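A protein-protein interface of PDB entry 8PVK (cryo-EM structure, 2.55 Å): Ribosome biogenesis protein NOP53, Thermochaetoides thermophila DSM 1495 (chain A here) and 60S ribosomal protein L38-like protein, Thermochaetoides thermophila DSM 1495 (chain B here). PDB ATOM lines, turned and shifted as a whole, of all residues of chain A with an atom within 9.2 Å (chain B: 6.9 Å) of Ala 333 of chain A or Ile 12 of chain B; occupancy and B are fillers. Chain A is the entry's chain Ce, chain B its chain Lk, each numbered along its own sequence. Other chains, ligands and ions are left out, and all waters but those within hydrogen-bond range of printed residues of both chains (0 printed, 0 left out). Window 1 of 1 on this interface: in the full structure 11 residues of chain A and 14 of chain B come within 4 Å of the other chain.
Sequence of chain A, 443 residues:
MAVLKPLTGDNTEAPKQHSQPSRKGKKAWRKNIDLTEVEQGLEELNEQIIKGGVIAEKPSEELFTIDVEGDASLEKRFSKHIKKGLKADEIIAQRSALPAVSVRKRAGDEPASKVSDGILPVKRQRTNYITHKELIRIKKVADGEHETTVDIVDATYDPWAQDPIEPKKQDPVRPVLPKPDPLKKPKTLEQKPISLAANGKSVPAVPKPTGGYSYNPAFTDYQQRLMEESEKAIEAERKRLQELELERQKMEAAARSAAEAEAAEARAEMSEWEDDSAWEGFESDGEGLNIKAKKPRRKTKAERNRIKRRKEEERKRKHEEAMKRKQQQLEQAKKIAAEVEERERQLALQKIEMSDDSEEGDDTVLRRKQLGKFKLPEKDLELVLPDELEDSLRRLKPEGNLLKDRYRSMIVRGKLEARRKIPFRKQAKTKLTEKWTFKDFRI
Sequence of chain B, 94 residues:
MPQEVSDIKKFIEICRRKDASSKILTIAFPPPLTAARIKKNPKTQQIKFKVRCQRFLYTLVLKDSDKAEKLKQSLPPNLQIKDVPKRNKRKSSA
OE1 of Gln 329 of chain A sits close to OD1 of Asp 7 of chain B (2.9 Å). The side-chain carboxylate of Glu 341 of chain A is in salt-bridge range of the guanidinium group of Arg 16 of chain B. The side-chain carboxylate (OE1) of Glu 344 of chain A lies within salt-bridge range of the guanidinium group (NE) of Arg 16 of chain B.
The side-chain carboxylate of Asp 7 of chain B lies within hydrogen-bond range of the backbone NH of Lys 9 of chain B, 3.2 Å away. OD2 of Asp 7 of chain B is in hydrogen-bond range of N of Lys 10 of chain B, at 2.8 Å.
Among the printed residues, merely in contact across the chains: Glu 331 of chain A with Lys 67 of chain B, Gln 329 of chain A with Ile 8 of chain B, Val 340 of chain A with Lys 9 of chain B, Lys 334 of chain A with Ser 74 of chain B, Ile 336 of chain A with Lys 9 of chain B, Lys 334 of chain A with Lys 70 of chain B, Leu 330 of chain A with Ile 8 of chain B, Ile 336 of chain A with Ile 12 of chain B, Ala 333 of chain A with Leu 71 of chain B, Ala 333 of chain A with Ile 12 of chain B, Leu 330 of chain A with Lys 67 of chain B, Ala 337 of chain A with Ile 12 of chain B, Val 340 of chain A with Arg 16 of chain B, Val 340 of chain A with Ile 12 of chain B and Ala 337 of chain A with Ser 74 of chain B.
Arg 325 of chain A touches none of the printed residues of chain B. Of chain B, only Ile 12 (3.9 Å) and Leu 71 (3.9 Å) come within 4 Å of Ala 333 of chain A. Of the printed residues of chain B, Val 340 of chain A touches Lys 9, Ile 12 and Arg 16. Of the printed residues of chain A, Ile 8 of chain B touches Gln 329 (3.5 Å) and Leu 330 (3.8 Å). Of chain A, only Ala 333 (3.9 Å), Ile 336 (3.9 Å), Ala 337 (3.9 Å) and Val 340 (3.97 Å) come within 4 Å of Ile 12 of chain B. No residue of chain A comes within 4 Å of Cys 15 of chain B. Of the printed residues of chain A, Arg 16 of chain B touches Val 340 (3.9 Å), Glu 341 (3.0 Å) and Glu 344 (2.6 Å). Printed residues of chain A within 4 Å of Ser 74 of chain B: Lys 334 and Ala 337. The nearest residue of chain A that does not touch Ile 12 of chain B is Lys 334 of chain A (6.0 Å). The nearest printed residue of chain A that does not touch Arg 16 of chain B is Ala 337 of chain A (5.9 Å).
Of the 18 printed residues of chain B, 9 touch a printed residue of chain A. Of the 18 printed residues of chain A, 10 touch a printed residue of chain B. Among the printed residues, 18 pairs touch across the chains.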
ATOM      1  N   ARG A 325     -28.524  27.287  18.909  1.00  0.00           N
ATOM      2  CA  ARG A 325     -28.480  26.964  20.337  1.00  0.00           C
ATOM      3  C   ARG A 325     -27.582  25.758  20.605  1.00  0.00           C
ATOM      4  O   ARG A 325     -26.910  25.703  21.645  1.00  0.00           O
ATOM      5  CB  ARG A 325     -29.882  26.738  20.927  1.00  0.00           C
ATOM      6  CG  ARG A 325     -30.630  25.508  20.448  1.00  0.00           C
ATOM      7  CD  ARG A 325     -32.007  25.355  21.088  1.00  0.00           C
ATOM      8  NE  ARG A 325     -32.954  26.411  20.751  1.00  0.00           N
ATOM      9  CZ  ARG A 325     -33.357  27.346  21.600  1.00  0.00           C
ATOM     10  NH1 ARG A 325     -32.886  27.406  22.835  1.00  0.00           N
ATOM     11  NH2 ARG A 325     -34.264  28.234  21.207  1.00  0.00           N
ATOM     12  N   LYS A 326     -27.530  24.798  19.671  1.00  0.00           N
ATOM     13  CA  LYS A 326     -26.598  23.682  19.829  1.00  0.00           C
ATOM     14  C   LYS A 326     -25.151  24.159  19.772  1.00  0.00           C
ATOM     15  O   LYS A 326     -24.305  23.695  20.549  1.00  0.00           O
ATOM     16  CB  LYS A 326     -26.854  22.615  18.765  1.00  0.00           C
ATOM     17  CG  LYS A 326     -25.991  21.372  18.945  1.00  0.00           C
ATOM     18  CD  LYS A 326     -26.632  20.128  18.353  1.00  0.00           C
ATOM     19  CE  LYS A 326     -26.718  20.211  16.841  1.00  0.00           C
ATOM     20  NZ  LYS A 326     -27.272  18.958  16.258  1.00  0.00           N
ATOM     21  N   GLN A 327     -24.851  25.097  18.867  1.00  0.00           N
ATOM     22  CA  GLN A 327     -23.501  25.650  18.793  1.00  0.00           C
ATOM     23  C   GLN A 327     -23.138  26.420  20.060  1.00  0.00           C
ATOM     24  O   GLN A 327     -22.002  26.332  20.540  1.00  0.00           O
ATOM     25  CB  GLN A 327     -23.369  26.547  17.562  1.00  0.00           C
ATOM     26  CG  GLN A 327     -21.949  27.012  17.283  1.00  0.00           C
ATOM     27  CD  GLN A 327     -21.026  25.874  16.892  1.00  0.00           C
ATOM     28  OE1 GLN A 327     -21.448  24.904  16.261  1.00  0.00           O
ATOM     29  NE2 GLN A 327     -19.756  25.986  17.265  1.00  0.00           N
ATOM     30  N   GLN A 328     -24.093  27.173  20.618  1.00  0.00           N
ATOM     31  CA  GLN A 328     -23.832  27.899  21.861  1.00  0.00           C
ATOM     32  C   GLN A 328     -23.571  26.946  23.025  1.00  0.00           C
ATOM     33  O   GLN A 328     -22.669  27.184  23.841  1.00  0.00           O
ATOM     34  CB  GLN A 328     -24.998  28.832  22.187  1.00  0.00           C
ATOM     35  CG  GLN A 328     -25.157  29.996  21.222  1.00  0.00           C
ATOM     36  CD  GLN A 328     -24.024  31.001  21.322  1.00  0.00           C
ATOM     37  OE1 GLN A 328     -23.406  31.156  22.375  1.00  0.00           O
ATOM     38  NE2 GLN A 328     -23.746  31.688  20.220  1.00  0.00           N
ATOM     39  N   GLN A 329     -24.344  25.858  23.115  1.00  0.00           N
ATOM     40  CA  GLN A 329     -24.104  24.865  24.161  1.00  0.00           C
ATOM     41  C   GLN A 329     -22.749  24.186  23.985  1.00  0.00           C
ATOM     42  O   GLN A 329     -22.056  23.904  24.973  1.00  0.00           O
ATOM     43  CB  GLN A 329     -25.225  23.829  24.175  1.00  0.00           C
ATOM     44  CG  GLN A 329     -26.547  24.347  24.712  1.00  0.00           C
ATOM     45  CD  GLN A 329     -27.671  23.346  24.544  1.00  0.00           C
ATOM     46  OE1 GLN A 329     -27.504  22.314  23.896  1.00  0.00           O
ATOM     47  NE2 GLN A 329     -28.823  23.646  25.131  1.00  0.00           N
ATOM     48  N   LEU A 330     -22.355  23.918  22.736  1.00  0.00           N
ATOM     49  CA  LEU A 330     -21.027  23.368  22.476  1.00  0.00           C
ATOM     50  C   LEU A 330     -19.932  24.341  22.898  1.00  0.00           C
ATOM     51  O   LEU A 330     -18.874  23.924  23.384  1.00  0.00           O
ATOM     52  CB  LEU A 330     -20.889  23.008  20.997  1.00  0.00           C
ATOM     53  CG  LEU A 330     -19.561  22.386  20.564  1.00  0.00           C
ATOM     54  CD1 LEU A 330     -19.349  21.048  21.252  1.00  0.00           C
ATOM     55  CD2 LEU A 330     -19.509  22.231  19.054  1.00  0.00           C
ATOM     56  N   GLU A 331     -20.166  25.643  22.711  1.00  0.00           N
ATOM     57  CA  GLU A 331     -19.209  26.642  23.183  1.00  0.00           C
ATOM     58  C   GLU A 331     -19.104  26.645  24.706  1.00  0.00           C
ATOM     59  O   GLU A 331     -18.003  26.757  25.256  1.00  0.00           O
ATOM     60  CB  GLU A 331     -19.595  28.031  22.673  1.00  0.00           C
ATOM     61  CG  GLU A 331     -19.425  28.222  21.172  1.00  0.00           C
ATOM     62  CD  GLU A 331     -17.975  28.190  20.734  1.00  0.00           C
ATOM     63  OE1 GLU A 331     -17.101  28.612  21.520  1.00  0.00           O
ATOM     64  OE2 GLU A 331     -17.707  27.747  19.597  1.00  0.00           O
ATOM     65  N   GLN A 332     -20.235  26.525  25.406  1.00  0.00           N
ATOM     66  CA  GLN A 332     -20.235  26.532  26.868  1.00  0.00           C
ATOM     67  C   GLN A 332     -20.308  25.125  27.467  1.00  0.00           C
ATOM     68  O   GLN A 332     -20.854  24.944  28.561  1.00  0.00           O
ATOM     69  CB  GLN A 332     -21.372  27.406  27.404  1.00  0.00           C
ATOM     70  CG  GLN A 332     -22.779  26.960  27.032  1.00  0.00           C
ATOM     71  CD  GLN A 332     -23.847  27.719  27.792  1.00  0.00           C
ATOM     72  OE1 GLN A 332     -23.819  28.947  27.866  1.00  0.00           O
ATOM     73  NE2 GLN A 332     -24.798  26.989  28.363  1.00  0.00           N
ATOM     74  N   ALA A 333     -19.739  24.131  26.774  1.00  0.00           N
ATOM     75  CA  ALA A 333     -19.844  22.735  27.200  1.00  0.00           C
ATOM     76  C   ALA A 333     -19.168  22.468  28.545  1.00  0.00           C
ATOM     77  O   ALA A 333     -19.629  21.611  29.309  1.00  0.00           O
ATOM     78  CB  ALA A 333     -19.254  21.822  26.125  1.00  0.00           C
ATOM     79  N   LYS A 334     -18.062  23.161  28.844  1.00  0.00           N
ATOM     80  CA  LYS A 334     -17.320  22.879  30.076  1.00  0.00           C
ATOM     81  C   LYS A 334     -18.116  23.261  31.322  1.00  0.00           C
ATOM     82  O   LYS A 334     -18.118  22.520  32.317  1.00  0.00           O
ATOM     83  CB  LYS A 334     -15.975  23.603  30.062  1.00  0.00           C
ATOM     84  CG  LYS A 334     -14.996  23.089  29.020  1.00  0.00           C
ATOM     85  CD  LYS A 334     -13.574  23.514  29.356  1.00  0.00           C
ATOM     86  CE  LYS A 334     -12.568  22.432  28.995  1.00  0.00           C
ATOM     87  NZ  LYS A 334     -12.703  21.996  27.578  1.00  0.00           N
ATOM     88  N   LYS A 335     -18.792  24.414  31.289  1.00  0.00           N
ATOM     89  CA  LYS A 335     -19.652  24.811  32.399  1.00  0.00           C
ATOM     90  C   LYS A 335     -20.814  23.840  32.564  1.00  0.00           C
ATOM     91  O   LYS A 335     -21.241  23.554  33.689  1.00  0.00           O
ATOM     92  CB  LYS A 335     -20.171  26.230  32.176  1.00  0.00           C
ATOM     93  CG  LYS A 335     -19.111  27.311  32.287  1.00  0.00           C
ATOM     94  CD  LYS A 335     -19.682  28.667  31.911  1.00  0.00           C
ATOM     95  CE  LYS A 335     -20.655  29.168  32.965  1.00  0.00           C
ATOM     96  NZ  LYS A 335     -21.133  30.546  32.666  1.00  0.00           N
ATOM     97  N   ILE A 336     -21.330  23.323  31.447  1.00  0.00           N
ATOM     98  CA  ILE A 336     -22.387  22.317  31.484  1.00  0.00           C
ATOM     99  C   ILE A 336     -21.897  21.044  32.163  1.00  0.00           C
ATOM    100  O   ILE A 336     -22.607  20.447  32.984  1.00  0.00           O
ATOM    101  CB  ILE A 336     -22.893  22.042  30.056  1.00  0.00           C
ATOM    102  CG1 ILE A 336     -23.562  23.290  29.478  1.00  0.00           C
ATOM    103  CG2 ILE A 336     -23.838  20.869  30.041  1.00  0.00           C
ATOM    104  CD1 ILE A 336     -23.988  23.135  28.038  1.00  0.00           C
ATOM    105  N   ALA A 337     -20.672  20.617  31.838  1.00  0.00           N
ATOM    106  CA  ALA A 337     -20.093  19.443  32.483  1.00  0.00           C
ATOM    107  C   ALA A 337     -19.919  19.666  33.979  1.00  0.00           C
ATOM    108  O   ALA A 337     -20.200  18.769  34.784  1.00  0.00           O
ATOM    109  CB  ALA A 337     -18.753  19.096  31.835  1.00  0.00           C
ATOM    110  N   ALA A 338     -19.478  20.867  34.368  1.00  0.00           N
ATOM    111  CA  ALA A 338     -19.324  21.184  35.786  1.00  0.00           C
ATOM    112  C   ALA A 338     -20.665  21.177  36.512  1.00  0.00           C
ATOM    113  O   ALA A 338     -20.757  20.719  37.657  1.00  0.00           O
ATOM    114  CB  ALA A 338     -18.634  22.536  35.949  1.00  0.00           C
ATOM    115  N   GLU A 339     -21.717  21.687  35.865  1.00  0.00           N
ATOM    116  CA  GLU A 339     -23.043  21.688  36.480  1.00  0.00           C
ATOM    117  C   GLU A 339     -23.602  20.275  36.620  1.00  0.00           C
ATOM    118  O   GLU A 339     -24.247  19.956  37.626  1.00  0.00           O
ATOM    119  CB  GLU A 339     -23.999  22.563  35.670  1.00  0.00           C
ATOM    120  CG  GLU A 339     -23.719  24.051  35.770  1.00  0.00           C
ATOM    121  CD  GLU A 339     -24.315  24.826  34.612  1.00  0.00           C
ATOM    122  OE1 GLU A 339     -24.892  24.191  33.705  1.00  0.00           O
ATOM    123  OE2 GLU A 339     -24.203  26.070  34.608  1.00  0.00           O
ATOM    124  N   VAL A 340     -23.371  19.420  35.617  1.00  0.00           N
ATOM    125  CA  VAL A 340     -23.761  18.014  35.714  1.00  0.00           C
ATOM    126  C   VAL A 340     -23.023  17.327  36.862  1.00  0.00           C
ATOM    127  O   VAL A 340     -23.623  16.566  37.637  1.00  0.00           O
ATOM    128  CB  VAL A 340     -23.515  17.306  34.368  1.00  0.00           C
ATOM    129  CG1 VAL A 340     -23.621  15.793  34.524  1.00  0.00           C
ATOM    130  CG2 VAL A 340     -24.508  17.803  33.314  1.00  0.00           C
ATOM    131  N   GLU A 341     -21.713  17.604  36.994  1.00  0.00           N
ATOM    132  CA  GLU A 341     -20.917  17.119  38.127  1.00  0.00           C
ATOM    133  C   GLU A 341     -21.494  17.584  39.462  1.00  0.00           C
ATOM    134  O   GLU A 341     -21.592  16.795  40.413  1.00  0.00           O
ATOM    135  CB  GLU A 341     -19.463  17.601  37.983  1.00  0.00           C
ATOM    136  CG  GLU A 341     -18.613  16.891  36.924  1.00  0.00           C
ATOM    137  CD  GLU A 341     -18.253  15.487  37.306  1.00  0.00           C
ATOM    138  OE1 GLU A 341     -18.890  14.567  36.762  1.00  0.00           O
ATOM    139  OE2 GLU A 341     -17.266  15.304  38.066  1.00  0.00           O
ATOM    140  N   GLU A 344     -24.826  15.674  40.160  1.00  0.00           N
ATOM    141  CA  GLU A 344     -24.588  14.291  40.565  1.00  0.00           C
ATOM    142  C   GLU A 344     -24.013  14.212  41.974  1.00  0.00           C
ATOM    143  O   GLU A 344     -24.386  13.325  42.753  1.00  0.00           O
ATOM    144  CB  GLU A 344     -23.667  13.587  39.569  1.00  0.00           C
ATOM    145  CG  GLU A 344     -24.336  13.243  38.249  1.00  0.00           C
ATOM    146  CD  GLU A 344     -23.476  12.360  37.364  1.00  0.00           C
ATOM    147  OE1 GLU A 344     -22.301  12.122  37.716  1.00  0.00           O
ATOM    148  OE2 GLU A 344     -23.980  11.897  36.319  1.00  0.00           O
ATOM    149  N   VAL B   5     -29.067  12.666  19.730  1.00  0.00           N
ATOM    150  CA  VAL B   5     -29.154  13.632  20.817  1.00  0.00           C
ATOM    151  C   VAL B   5     -28.827  15.008  20.263  1.00  0.00           C
ATOM    152  O   VAL B   5     -27.778  15.201  19.636  1.00  0.00           O
ATOM    153  CB  VAL B   5     -28.204  13.261  21.968  1.00  0.00           C
ATOM    154  CG1 VAL B   5     -28.427  14.180  23.153  1.00  0.00           C
ATOM    155  CG2 VAL B   5     -28.399  11.809  22.368  1.00  0.00           C
ATOM    156  N   ASP B   7     -28.826  17.763  22.332  1.00  0.00           N
ATOM    157  CA  ASP B   7     -28.473  18.585  23.480  1.00  0.00           C
ATOM    158  C   ASP B   7     -27.143  18.119  24.053  1.00  0.00           C
ATOM    159  O   ASP B   7     -26.963  16.928  24.336  1.00  0.00           O
ATOM    160  CB  ASP B   7     -29.569  18.527  24.548  1.00  0.00           C
ATOM    161  CG  ASP B   7     -29.170  19.225  25.833  1.00  0.00           C
ATOM    162  OD1 ASP B   7     -28.539  20.300  25.761  1.00  0.00           O
ATOM    163  OD2 ASP B   7     -29.496  18.701  26.918  1.00  0.00           O
ATOM    164  N   ILE B   8     -26.219  19.068  24.230  1.00  0.00           N
ATOM    165  CA  ILE B   8     -24.902  18.747  24.771  1.00  0.00           C
ATOM    166  C   ILE B   8     -25.015  18.302  26.223  1.00  0.00           C
ATOM    167  O   ILE B   8     -24.299  17.397  26.664  1.00  0.00           O
ATOM    168  CB  ILE B   8     -23.958  19.953  24.617  1.00  0.00           C
ATOM    169  CG1 ILE B   8     -24.010  20.488  23.184  1.00  0.00           C
ATOM    170  CG2 ILE B   8     -22.531  19.575  24.991  1.00  0.00           C
ATOM    171  CD1 ILE B   8     -23.383  19.574  22.161  1.00  0.00           C
ATOM    172  N   LYS B   9     -25.923  18.920  26.985  1.00  0.00           N
ATOM    173  CA  LYS B   9     -26.127  18.530  28.377  1.00  0.00           C
ATOM    174  C   LYS B   9     -26.671  17.110  28.482  1.00  0.00           C
ATOM    175  O   LYS B   9     -26.215  16.316  29.319  1.00  0.00           O
ATOM    176  CB  LYS B   9     -27.075  19.518  29.055  1.00  0.00           C
ATOM    177  CG  LYS B   9     -27.315  19.245  30.527  1.00  0.00           C
ATOM    178  CD  LYS B   9     -28.172  20.333  31.146  1.00  0.00           C
ATOM    179  CE  LYS B   9     -28.540  19.995  32.579  1.00  0.00           C
ATOM    180  NZ  LYS B   9     -27.342  19.978  33.461  1.00  0.00           N
ATOM    181  N   LYS B  10     -27.645  16.775  27.632  1.00  0.00           N
ATOM    182  CA  LYS B  10     -28.198  15.426  27.623  1.00  0.00           C
ATOM    183  C   LYS B  10     -27.150  14.409  27.190  1.00  0.00           C
ATOM    184  O   LYS B  10     -27.086  13.307  27.744  1.00  0.00           O
ATOM    185  CB  LYS B  10     -29.427  15.374  26.717  1.00  0.00           C
ATOM    186  CG  LYS B  10     -30.148  14.035  26.698  1.00  0.00           C
ATOM    187  CD  LYS B  10     -31.385  14.101  25.814  1.00  0.00           C
ATOM    188  CE  LYS B  10     -32.177  12.804  25.852  1.00  0.00           C
ATOM    189  NZ  LYS B  10     -31.448  11.673  25.222  1.00  0.00           N
ATOM    190  N   PHE B  11     -26.304  14.771  26.220  1.00  0.00           N
ATOM    191  CA  PHE B  11     -25.226  13.872  25.812  1.00  0.00           C
ATOM    192  C   PHE B  11     -24.194  13.684  26.920  1.00  0.00           C
ATOM    193  O   PHE B  11     -23.643  12.590  27.076  1.00  0.00           O
ATOM    194  CB  PHE B  11     -24.558  14.385  24.539  1.00  0.00           C
ATOM    195  CG  PHE B  11     -23.701  13.360  23.861  1.00  0.00           C
ATOM    196  CD1 PHE B  11     -24.278  12.291  23.196  1.00  0.00           C
ATOM    197  CD2 PHE B  11     -22.321  13.460  23.893  1.00  0.00           C
ATOM    198  CE1 PHE B  11     -23.495  11.338  22.576  1.00  0.00           C
ATOM    199  CE2 PHE B  11     -21.532  12.513  23.271  1.00  0.00           C
ATOM    200  CZ  PHE B  11     -22.121  11.448  22.616  1.00  0.00           C
ATOM    201  N   ILE B  12     -23.920  14.735  27.696  1.00  0.00           N
ATOM    202  CA  ILE B  12     -22.989  14.619  28.818  1.00  0.00           C
ATOM    203  C   ILE B  12     -23.553  13.690  29.891  1.00  0.00           C
ATOM    204  O   ILE B  12     -22.839  12.828  30.423  1.00  0.00           O
ATOM    205  CB  ILE B  12     -22.657  16.018  29.371  1.00  0.00           C
ATOM    206  CG1 ILE B  12     -21.670  16.731  28.442  1.00  0.00           C
ATOM    207  CG2 ILE B  12     -22.086  15.942  30.781  1.00  0.00           C
ATOM    208  CD1 ILE B  12     -21.341  18.145  28.859  1.00  0.00           C
ATOM    209  N   GLU B  13     -24.848  13.824  30.201  1.00  0.00           N
ATOM    210  CA  GLU B  13     -25.468  12.915  31.166  1.00  0.00           C
ATOM    211  C   GLU B  13     -25.504  11.478  30.648  1.00  0.00           C
ATOM    212  O   GLU B  13     -25.314  10.529  31.423  1.00  0.00           O
ATOM    213  CB  GLU B  13     -26.878  13.387  31.520  1.00  0.00           C
ATOM    214  CG  GLU B  13     -26.928  14.693  32.292  1.00  0.00           C
ATOM    215  CD  GLU B  13     -28.346  15.127  32.606  1.00  0.00           C
ATOM    216  OE1 GLU B  13     -29.293  14.477  32.115  1.00  0.00           O
ATOM    217  OE2 GLU B  13     -28.516  16.114  33.352  1.00  0.00           O
ATOM    218  N   ILE B  14     -25.746  11.297  29.346  1.00  0.00           N
ATOM    219  CA  ILE B  14     -25.752   9.957  28.763  1.00  0.00           C
ATOM    220  C   ILE B  14     -24.361   9.334  28.829  1.00  0.00           C
ATOM    221  O   ILE B  14     -24.211   8.154  29.171  1.00  0.00           O
ATOM    222  CB  ILE B  14     -26.297  10.011  27.323  1.00  0.00           C
ATOM    223  CG1 ILE B  14     -27.815  10.194  27.337  1.00  0.00           C
ATOM    224  CG2 ILE B  14     -25.955   8.752  26.558  1.00  0.00           C
ATOM    225  CD1 ILE B  14     -28.411  10.405  25.971  1.00  0.00           C
ATOM    226  N   CYS B  15     -23.321  10.118  28.531  1.00  0.00           N
ATOM    227  CA  CYS B  15     -21.955   9.620  28.658  1.00  0.00           C
ATOM    228  C   CYS B  15     -21.583   9.337  30.108  1.00  0.00           C
ATOM    229  O   CYS B  15     -20.721   8.490  30.367  1.00  0.00           O
ATOM    230  CB  CYS B  15     -20.965  10.611  28.044  1.00  0.00           C
ATOM    231  SG  CYS B  15     -21.037  10.716  26.247  1.00  0.00           S
ATOM    232  N   ARG B  16     -22.199  10.035  31.063  1.00  0.00           N
ATOM    233  CA  ARG B  16     -21.963   9.703  32.463  1.00  0.00           C
ATOM    234  C   ARG B  16     -22.913   8.653  33.025  1.00  0.00           C
ATOM    235  O   ARG B  16     -22.822   8.346  34.217  1.00  0.00           O
ATOM    236  CB  ARG B  16     -22.031  10.937  33.363  1.00  0.00           C
ATOM    237  CG  ARG B  16     -20.815  11.817  33.292  1.00  0.00           C
ATOM    238  CD  ARG B  16     -20.930  12.912  34.330  1.00  0.00           C
ATOM    239  NE  ARG B  16     -20.711  12.327  35.648  1.00  0.00           N
ATOM    240  CZ  ARG B  16     -19.607  11.712  36.055  1.00  0.00           C
ATOM    241  NH1 ARG B  16     -18.450  11.865  35.428  1.00  0.00           N
ATOM    242  NH2 ARG B  16     -19.653  10.966  37.154  1.00  0.00           N
ATOM    243  N   ARG B  17     -23.827   8.118  32.225  1.00  0.00           N
ATOM    244  CA  ARG B  17     -24.590   6.962  32.676  1.00  0.00           C
ATOM    245  C   ARG B  17     -23.671   5.755  32.853  1.00  0.00           C
ATOM    246  O   ARG B  17     -22.639   5.628  32.188  1.00  0.00           O
ATOM    247  CB  ARG B  17     -25.704   6.645  31.687  1.00  0.00           C
ATOM    248  CG  ARG B  17     -26.927   7.514  31.867  1.00  0.00           C
ATOM    249  CD  ARG B  17     -27.813   7.425  30.651  1.00  0.00           C
ATOM    250  NE  ARG B  17     -28.047   6.044  30.254  1.00  0.00           N
ATOM    251  CZ  ARG B  17     -28.885   5.681  29.293  1.00  0.00           C
ATOM    252  NH1 ARG B  17     -29.577   6.574  28.608  1.00  0.00           N
ATOM    253  NH2 ARG B  17     -29.024   4.390  29.007  1.00  0.00           N
ATOM    254  N   LYS B  67     -13.885  23.455  19.204  1.00  0.00           N
ATOM    255  CA  LYS B  67     -14.682  23.205  20.403  1.00  0.00           C
ATOM    256  C   LYS B  67     -15.300  21.809  20.375  1.00  0.00           C
ATOM    257  O   LYS B  67     -15.426  21.154  21.420  1.00  0.00           O
ATOM    258  CB  LYS B  67     -15.765  24.275  20.543  1.00  0.00           C
ATOM    259  CG  LYS B  67     -15.272  25.731  20.668  1.00  0.00           C
ATOM    260  CD  LYS B  67     -14.609  26.071  22.014  1.00  0.00           C
ATOM    261  CE  LYS B  67     -13.082  25.965  21.993  1.00  0.00           C
ATOM    262  NZ  LYS B  67     -12.474  26.407  23.279  1.00  0.00           N
ATOM    263  N   LYS B  70     -12.596  19.743  21.583  1.00  0.00           N
ATOM    264  CA  LYS B  70     -12.391  19.927  23.019  1.00  0.00           C
ATOM    265  C   LYS B  70     -13.521  19.360  23.868  1.00  0.00           C
ATOM    266  O   LYS B  70     -13.380  19.315  25.094  1.00  0.00           O
ATOM    267  CB  LYS B  70     -12.204  21.408  23.361  1.00  0.00           C
ATOM    268  CG  LYS B  70     -10.995  22.065  22.719  1.00  0.00           C
ATOM    269  CD  LYS B  70      -9.697  21.530  23.293  1.00  0.00           C
ATOM    270  CE  LYS B  70      -8.496  22.190  22.637  1.00  0.00           C
ATOM    271  NZ  LYS B  70      -8.396  23.632  22.992  1.00  0.00           N
ATOM    272  N   LEU B  71     -14.639  18.959  23.254  1.00  0.00           N
ATOM    273  CA  LEU B  71     -15.678  18.229  23.984  1.00  0.00           C
ATOM    274  C   LEU B  71     -15.163  16.914  24.578  1.00  0.00           C
ATOM    275  O   LEU B  71     -15.741  16.417  25.556  1.00  0.00           O
ATOM    276  CB  LEU B  71     -16.869  17.967  23.056  1.00  0.00           C
ATOM    277  CG  LEU B  71     -18.152  17.355  23.626  1.00  0.00           C
ATOM    278  CD1 LEU B  71     -18.743  18.246  24.706  1.00  0.00           C
ATOM    279  CD2 LEU B  71     -19.165  17.105  22.523  1.00  0.00           C
ATOM    280  N   SER B  74     -14.381  17.462  28.210  1.00  0.00           N
ATOM    281  CA  SER B  74     -15.560  17.437  29.065  1.00  0.00           C
ATOM    282  C   SER B  74     -16.146  16.040  29.204  1.00  0.00           C
ATOM    283  O   SER B  74     -16.841  15.771  30.191  1.00  0.00           O
ATOM    284  CB  SER B  74     -16.625  18.392  28.525  1.00  0.00           C
ATOM    285  OG  SER B  74     -16.144  19.723  28.490  1.00  0.00           O
ATOM    286  N   LEU B  75     -15.897  15.159  28.239  1.00  0.00           N
ATOM    287  CA  LEU B  75     -16.338  13.776  28.362  1.00  0.00           C
ATOM    288  C   LEU B  75     -15.582  13.068  29.491  1.00  0.00           C
ATOM    289  O   LEU B  75     -14.450  13.441  29.814  1.00  0.00           O
ATOM    290  CB  LEU B  75     -16.143  13.036  27.039  1.00  0.00           C
ATOM    291  CG  LEU B  75     -17.099  13.457  25.919  1.00  0.00           C
ATOM    292  CD1 LEU B  75     -16.951  12.557  24.707  1.00  0.00           C
ATOM    293  CD2 LEU B  75     -18.541  13.474  26.407  1.00  0.00           C
ATOM    294  N   PRO B  76     -16.204  12.065  30.131  1.00  0.00           N
ATOM    295  CA  PRO B  76     -15.578  11.441  31.301  1.00  0.00           C
ATOM    296  C   PRO B  76     -14.318  10.679  30.926  1.00  0.00           C
ATOM    297  O   PRO B  76     -14.191  10.177  29.797  1.00  0.00           O
ATOM    298  CB  PRO B  76     -16.669  10.487  31.818  1.00  0.00           C
ATOM    299  CG  PRO B  76     -17.926  11.030  31.289  1.00  0.00           C
ATOM    300  CD  PRO B  76     -17.598  11.618  29.959  1.00  0.00           C
